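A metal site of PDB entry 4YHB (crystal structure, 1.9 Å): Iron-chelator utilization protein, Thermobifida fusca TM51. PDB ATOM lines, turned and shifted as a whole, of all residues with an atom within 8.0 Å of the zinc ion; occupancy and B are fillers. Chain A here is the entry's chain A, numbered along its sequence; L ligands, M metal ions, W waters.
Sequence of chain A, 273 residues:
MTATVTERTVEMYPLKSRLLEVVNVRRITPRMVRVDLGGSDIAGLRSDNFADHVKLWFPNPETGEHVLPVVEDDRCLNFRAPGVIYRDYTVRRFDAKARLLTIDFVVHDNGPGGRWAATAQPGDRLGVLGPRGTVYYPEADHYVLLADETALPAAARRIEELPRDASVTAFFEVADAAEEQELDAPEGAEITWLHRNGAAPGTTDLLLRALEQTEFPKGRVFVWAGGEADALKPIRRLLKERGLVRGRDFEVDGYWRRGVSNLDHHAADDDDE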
ATOM      1  N   ALA A  51      -4.264 -16.556 -14.492  1.00  0.00           N
ATOM      2  CA  ALA A  51      -3.268 -15.498 -14.388  1.00  0.00           C
ATOM      3  C   ALA A  51      -3.267 -14.800 -13.035  1.00  0.00           C
ATOM      4  O   ALA A  51      -2.616 -13.758 -12.883  1.00  0.00           O
ATOM      5  CB  ALA A  51      -3.474 -14.484 -15.506  1.00  0.00           C
ATOM      6  N   ASP A  52      -3.979 -15.356 -12.062  1.00  0.00           N
ATOM      7  CA  ASP A  52      -3.962 -14.812 -10.694  1.00  0.00           C
ATOM      8  C   ASP A  52      -2.519 -14.663 -10.211  1.00  0.00           C
ATOM      9  O   ASP A  52      -1.682 -15.521 -10.460  1.00  0.00           O
ATOM     10  CB  ASP A  52      -4.719 -15.717  -9.718  1.00  0.00           C
ATOM     11  CG  ASP A  52      -6.225 -15.691  -9.926  1.00  0.00           C
ATOM     12  OD1 ASP A  52      -6.721 -14.882 -10.743  1.00  0.00           O
ATOM     13  OD2 ASP A  52      -6.899 -16.482  -9.229  1.00  0.00           O
ATOM     14  N   HIS A  53      -2.232 -13.560  -9.531  1.00  0.00           N
ATOM     15  CA  HIS A  53      -0.864 -13.341  -9.066  1.00  0.00           C
ATOM     16  C   HIS A  53      -0.834 -12.613  -7.734  1.00  0.00           C
ATOM     17  O   HIS A  53      -1.717 -11.827  -7.397  1.00  0.00           O
ATOM     18  CB  HIS A  53      -0.048 -12.562 -10.106  1.00  0.00           C
ATOM     19  CG  HIS A  53      -0.707 -11.294 -10.553  1.00  0.00           C
ATOM     20  ND1 HIS A  53      -1.725 -11.279 -11.484  1.00  0.00           N
ATOM     21  CD2 HIS A  53      -0.507 -10.001 -10.196  1.00  0.00           C
ATOM     22  CE1 HIS A  53      -2.112 -10.033 -11.691  1.00  0.00           C
ATOM     23  NE2 HIS A  53      -1.390  -9.242 -10.911  1.00  0.00           N
ATOM     24  N   VAL A  54       0.227 -12.885  -6.977  1.00  0.00           N
ATOM     25  CA  VAL A  54       0.436 -12.245  -5.686  1.00  0.00           C
ATOM     26  C   VAL A  54       1.632 -11.325  -5.792  1.00  0.00           C
ATOM     27  O   VAL A  54       2.389 -11.373  -6.767  1.00  0.00           O
ATOM     28  CB  VAL A  54       0.688 -13.288  -4.570  1.00  0.00           C
ATOM     29  CG1 VAL A  54      -0.546 -14.100  -4.316  1.00  0.00           C
ATOM     30  CG2 VAL A  54       1.868 -14.204  -4.926  1.00  0.00           C
ATOM     31  N   LYS A  55       1.798 -10.469  -4.788  1.00  0.00           N
ATOM     32  CA  LYS A  55       3.063  -9.772  -4.624  1.00  0.00           C
ATOM     33  C   LYS A  55       3.807 -10.470  -3.506  1.00  0.00           C
ATOM     34  O   LYS A  55       3.296 -10.626  -2.394  1.00  0.00           O
ATOM     35  CB  LYS A  55       2.855  -8.285  -4.292  1.00  0.00           C
ATOM     36  CG  LYS A  55       2.624  -7.390  -5.520  1.00  0.00           C
ATOM     37  CD  LYS A  55       2.034  -6.032  -5.121  1.00  0.00           C
ATOM     38  CE  LYS A  55       2.200  -5.021  -6.239  1.00  0.00           C
ATOM     39  NZ  LYS A  55       1.667  -5.502  -7.549  1.00  0.00           N
ATOM     40  N   ASP A  88       5.786  -9.164  -8.452  1.00  0.00           N
ATOM     41  CA  ASP A  88       4.640  -9.953  -8.905  1.00  0.00           C
ATOM     42  C   ASP A  88       5.054 -11.364  -9.293  1.00  0.00           C
ATOM     43  O   ASP A  88       5.969 -11.531 -10.111  1.00  0.00           O
ATOM     44  CB  ASP A  88       3.978  -9.311 -10.122  1.00  0.00           C
ATOM     45  CG  ASP A  88       3.099  -8.147  -9.769  1.00  0.00           C
ATOM     46  OD1 ASP A  88       3.191  -7.626  -8.637  1.00  0.00           O
ATOM     47  OD2 ASP A  88       2.320  -7.733 -10.642  1.00  0.00           O
ATOM     48  N   PRO A 131      -3.936 -12.505  -3.976  1.00  0.00           N
ATOM     49  CA  PRO A 131      -4.205 -11.707  -5.181  1.00  0.00           C
ATOM     50  C   PRO A 131      -5.225 -10.616  -4.890  1.00  0.00           C
ATOM     51  O   PRO A 131      -6.066 -10.806  -4.036  1.00  0.00           O
ATOM     52  CB  PRO A 131      -4.785 -12.727  -6.167  1.00  0.00           C
ATOM     53  CG  PRO A 131      -4.426 -14.054  -5.625  1.00  0.00           C
ATOM     54  CD  PRO A 131      -4.409 -13.896  -4.136  1.00  0.00           C
ATOM     55  N   ARG A 132      -5.100  -9.480  -5.573  1.00  0.00           N
ATOM     56  CA  ARG A 132      -6.026  -8.367  -5.402  1.00  0.00           C
ATOM     57  C   ARG A 132      -7.419  -8.793  -5.856  1.00  0.00           C
ATOM     58  O   ARG A 132      -8.451  -8.311  -5.357  1.00  0.00           O
ATOM     59  CB  ARG A 132      -5.506  -7.159  -6.180  1.00  0.00           C
ATOM     60  CG  ARG A 132      -6.461  -5.953  -6.242  1.00  0.00           C
ATOM     61  CD  ARG A 132      -6.636  -5.271  -4.898  1.00  0.00           C
ATOM     62  NE  ARG A 132      -7.678  -5.887  -4.068  1.00  0.00           N
ATOM     63  CZ  ARG A 132      -8.177  -5.312  -2.978  1.00  0.00           C
ATOM     64  NH1 ARG A 132      -7.724  -4.123  -2.607  1.00  0.00           N
ATOM     65  NH2 ARG A 132      -9.121  -5.921  -2.255  1.00  0.00           N
ATOM     66  N   GLY A 133      -7.443  -9.711  -6.804  1.00  0.00           N
ATOM     67  CA  GLY A 133      -8.685 -10.205  -7.378  1.00  0.00           C
ATOM     68  C   GLY A 133      -8.395 -11.186  -8.498  1.00  0.00           C
ATOM     69  O   GLY A 133      -7.297 -11.744  -8.571  1.00  0.00           O
ATOM     70  N   ASP A 253       0.069  -8.957 -21.955  1.00  0.00           N
ATOM     71  CA  ASP A 253       0.435  -8.445 -20.631  1.00  0.00           C
ATOM     72  C   ASP A 253       1.941  -8.502 -20.463  1.00  0.00           C
ATOM     73  O   ASP A 253       2.541  -9.588 -20.439  1.00  0.00           O
ATOM     74  CB  ASP A 253      -0.279  -9.261 -19.542  1.00  0.00           C
ATOM     75  CG  ASP A 253      -0.404  -8.494 -18.205  1.00  0.00           C
ATOM     76  OD1 ASP A 253       0.223  -7.433 -18.056  1.00  0.00           O
ATOM     77  OD2 ASP A 253      -1.133  -8.970 -17.307  1.00  0.00           O
ATOM     78  N   TYR A 255       5.062  -8.628 -18.435  1.00  0.00           N
ATOM     79  CA  TYR A 255       5.373  -9.092 -17.072  1.00  0.00           C
ATOM     80  C   TYR A 255       6.677  -8.503 -16.515  1.00  0.00           C
ATOM     81  O   TYR A 255       6.880  -8.428 -15.307  1.00  0.00           O
ATOM     82  CB  TYR A 255       5.439 -10.620 -17.045  1.00  0.00           C
ATOM     83  CG  TYR A 255       4.080 -11.280 -16.868  1.00  0.00           C
ATOM     84  CD1 TYR A 255       2.902 -10.560 -17.039  1.00  0.00           C
ATOM     85  CD2 TYR A 255       3.984 -12.604 -16.480  1.00  0.00           C
ATOM     86  CE1 TYR A 255       1.664 -11.155 -16.855  1.00  0.00           C
ATOM     87  CE2 TYR A 255       2.733 -13.217 -16.297  1.00  0.00           C
ATOM     88  CZ  TYR A 255       1.584 -12.483 -16.494  1.00  0.00           C
ATOM     89  OH  TYR A 255       0.360 -13.077 -16.313  1.00  0.00           O
ATOM     90  N   ASP A 264       5.563  -2.232 -13.145  1.00  0.00           N
ATOM     91  CA  ASP A 264       4.160  -2.237 -12.738  1.00  0.00           C
ATOM     92  C   ASP A 264       3.278  -2.510 -13.946  1.00  0.00           C
ATOM     93  O   ASP A 264       3.125  -1.661 -14.813  1.00  0.00           O
ATOM     94  CB  ASP A 264       3.781  -0.901 -12.078  1.00  0.00           C
ATOM     95  CG  ASP A 264       2.328  -0.852 -11.586  1.00  0.00           C
ATOM     96  OD1 ASP A 264       1.527  -1.802 -11.817  1.00  0.00           O
ATOM     97  OD2 ASP A 264       1.984   0.165 -10.945  1.00  0.00           O
ATOM     98  N   HIS A 265       2.674  -3.690 -14.008  1.00  0.00           N
ATOM     99  CA  HIS A 265       1.945  -4.040 -15.216  1.00  0.00           C
ATOM    100  C   HIS A 265       0.540  -3.427 -15.246  1.00  0.00           C
ATOM    101  O   HIS A 265      -0.183  -3.549 -16.236  1.00  0.00           O
ATOM    102  CB  HIS A 265       1.891  -5.566 -15.375  1.00  0.00           C
ATOM    103  CG  HIS A 265       0.860  -6.237 -14.519  1.00  0.00           C
ATOM    104  ND1 HIS A 265       0.006  -7.202 -14.998  1.00  0.00           N
ATOM    105  CD2 HIS A 265       0.531  -6.060 -13.216  1.00  0.00           C
ATOM    106  CE1 HIS A 265      -0.781  -7.622 -14.024  1.00  0.00           C
ATOM    107  NE2 HIS A 265      -0.503  -6.919 -12.940  1.00  0.00           N
ATOM    108  N   HIS A 266       0.157  -2.736 -14.181  1.00  0.00           N
ATOM    109  CA  HIS A 266      -1.135  -2.051 -14.143  1.00  0.00           C
ATOM    110  C   HIS A 266      -1.120  -0.765 -14.962  1.00  0.00           C
ATOM    111  O   HIS A 266      -2.150  -0.353 -15.488  1.00  0.00           O
ATOM    112  CB  HIS A 266      -1.554  -1.759 -12.697  1.00  0.00           C
ATOM    113  CG  HIS A 266      -1.756  -2.993 -11.880  1.00  0.00           C
ATOM    114  ND1 HIS A 266      -1.610  -3.004 -10.515  1.00  0.00           N
ATOM    115  CD2 HIS A 266      -2.112  -4.247 -12.234  1.00  0.00           C
ATOM    116  CE1 HIS A 266      -1.849  -4.218 -10.054  1.00  0.00           C
ATOM    117  NE2 HIS A 266      -2.173  -4.991 -11.080  1.00  0.00           N
HETATM  118  P1  LIG L   1      13.970  -6.894 -10.661  1.00  0.00           P
HETATM  119  O1  LIG L   1      14.567  -6.127  -9.474  1.00  0.00           O
HETATM  120  O2  LIG L   1      12.452  -6.513 -10.896  1.00  0.00           O
HETATM  121  O3  LIG L   1      14.729  -6.405 -11.997  1.00  0.00           O
HETATM  122  C1  LIG L   1      16.104  -6.254 -11.998  1.00  0.00           C
HETATM  123  C2  LIG L   1      16.634  -6.445 -13.437  1.00  0.00           C
HETATM  124  O4  LIG L   1      16.504  -7.769 -13.875  1.00  0.00           O
HETATM  125  C3  LIG L   1      15.941  -5.603 -14.425  1.00  0.00           C
HETATM  126  O5  LIG L   1      16.909  -5.170 -15.312  1.00  0.00           O
HETATM  127  C4  LIG L   1      15.028  -6.485 -15.057  1.00  0.00           C
HETATM  128  O6  LIG L   1      14.779  -6.176 -16.423  1.00  0.00           O
HETATM  129  C5  LIG L   1      15.707  -7.784 -15.017  1.00  0.00           C
HETATM  130  N1  LIG L   1      14.827  -8.949 -14.949  1.00  0.00           N
HETATM  131  C6  LIG L   1      13.697  -9.066 -14.234  1.00  0.00           C
HETATM  132  N2  LIG L   1      13.197 -10.294 -14.424  1.00  0.00           N
HETATM  133  C7  LIG L   1      14.038 -10.976 -15.224  1.00  0.00           C
HETATM  134  C8  LIG L   1      14.059 -12.267 -15.754  1.00  0.00           C
HETATM  135  N3  LIG L   1      13.015 -13.177 -15.441  1.00  0.00           N
HETATM  136  N4  LIG L   1      15.073 -12.642 -16.555  1.00  0.00           N
HETATM  137  C9  LIG L   1      16.073 -11.788 -16.859  1.00  0.00           C
HETATM  138  N5  LIG L   1      16.090 -10.546 -16.370  1.00  0.00           N
HETATM  139  C10 LIG L   1      15.079 -10.117 -15.568  1.00  0.00           C
HETATM  140  N6  LIG L   1       8.167 -14.147 -12.886  1.00  0.00           N
HETATM  141  C11 LIG L   1       8.424 -15.414 -12.563  1.00  0.00           C
HETATM  142  O7  LIG L   1       9.584 -15.817 -12.545  1.00  0.00           O
HETATM  143  N7  LIG L   1       7.374 -16.235 -12.250  1.00  0.00           N
HETATM  144  C12 LIG L   1       6.096 -15.794 -12.261  1.00  0.00           C
HETATM  145  O8  LIG L   1       5.206 -16.572 -11.966  1.00  0.00           O
HETATM  146  C13 LIG L   1       5.801 -14.474 -12.603  1.00  0.00           C
HETATM  147  N8  LIG L   1       4.515 -13.969 -12.629  1.00  0.00           N
HETATM  148  C14 LIG L   1       4.299 -12.665 -12.953  1.00  0.00           C
HETATM  149  C15 LIG L   1       3.005 -12.149 -12.978  1.00  0.00           C
HETATM  150  C16 LIG L   1       2.793 -10.957 -13.264  1.00  0.00           C
HETATM  151  C17 LIG L   1       1.321 -10.504 -13.259  1.00  0.00           C
HETATM  152  C18 LIG L   1       3.641 -10.097 -13.556  1.00  0.00           C
HETATM  153  C19 LIG L   1       3.335  -8.672 -13.910  1.00  0.00           C
HETATM  154  C20 LIG L   1       4.970 -10.440 -13.571  1.00  0.00           C
HETATM  155  C21 LIG L   1       5.497 -11.839 -13.260  1.00  0.00           C
HETATM  156  N9  LIG L   1       6.711 -12.351 -13.234  1.00  0.00           N
HETATM  157  C22 LIG L   1       6.903 -13.653 -12.916  1.00  0.00           C
HETATM  158  C23 LIG L   1       7.870 -11.489 -13.565  1.00  0.00           C
HETATM  159  C24 LIG L   1       8.547 -10.918 -12.356  1.00  0.00           C
HETATM  160  O9  LIG L   1       7.654 -10.133 -11.671  1.00  0.00           O
HETATM  161  C25 LIG L   1       9.788 -10.091 -12.840  1.00  0.00           C
HETATM  162  O10 LIG L   1      10.591 -10.950 -13.586  1.00  0.00           O
HETATM  163  C26 LIG L   1      10.533  -9.361 -11.750  1.00  0.00           C
HETATM  164  O11 LIG L   1      11.256  -8.342 -12.293  1.00  0.00           O
HETATM  165  C27 LIG L   1      11.532 -10.250 -10.993  1.00  0.00           C
HETATM  166  O12 LIG L   1      11.955  -9.690  -9.776  1.00  0.00           O
HETATM  167  P2  LIG L   1      13.515  -9.461  -9.626  1.00  0.00           P
HETATM  168  O13 LIG L   1      13.607  -8.789  -8.239  1.00  0.00           O
HETATM  169  O14 LIG L   1      14.141 -10.833  -9.972  1.00  0.00           O
HETATM  170  O15 LIG L   1      14.369  -8.431 -10.463  1.00  0.00           O
HETATM  171 ZN    ZN M   1      -1.696  -7.099 -11.133  1.00  0.00          ZN
HETATM  172  O   HOH W   1       0.089  -6.765  -9.944  1.00  0.00           O
HETATM  173  O   HOH W   2      -2.845  -7.098  -9.179  1.00  0.00           O
HETATM  174  O   HOH W   3      -3.590  -7.469 -12.151  1.00  0.00           O
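O of Asp 88 is in hydrogen-bond range of O9 of the ligand.
Of the 14 residues printed, 3 come within 4 Å of the zinc ion. The nearest printed residue that does not touch the zinc ion is Asp 88 (4.1 Å).
OD1 of Asp 264 lies within hydrogen-bond range of N of His 266, 2.9 Å away. The side-chain carboxylate of Asp 253 sits at hydrogen-bond distance from a ring nitrogen (ND1) of His 265 (3.1 Å). A ring nitrogen (ND1) of His 53 lies within hydrogen-bond range of the backbone carbonyl oxygen (O) of Ala 51 (3.0 Å).
Water W1 bridges the side-chain carboxylate (OD2) of Asp 88 and the side-chain amino group (NZ) of Lys 55.
The zinc ion is bound by a ring nitrogen (NE2) of His 266 (2.2 Å), water W1 (2.2 Å), a ring nitrogen (NE2) of His 265 (2.2 Å), a ring nitrogen (NE2) of His 53 (2.2 Å), water W3 (2.2 Å) and water W2 (2.3 Å).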
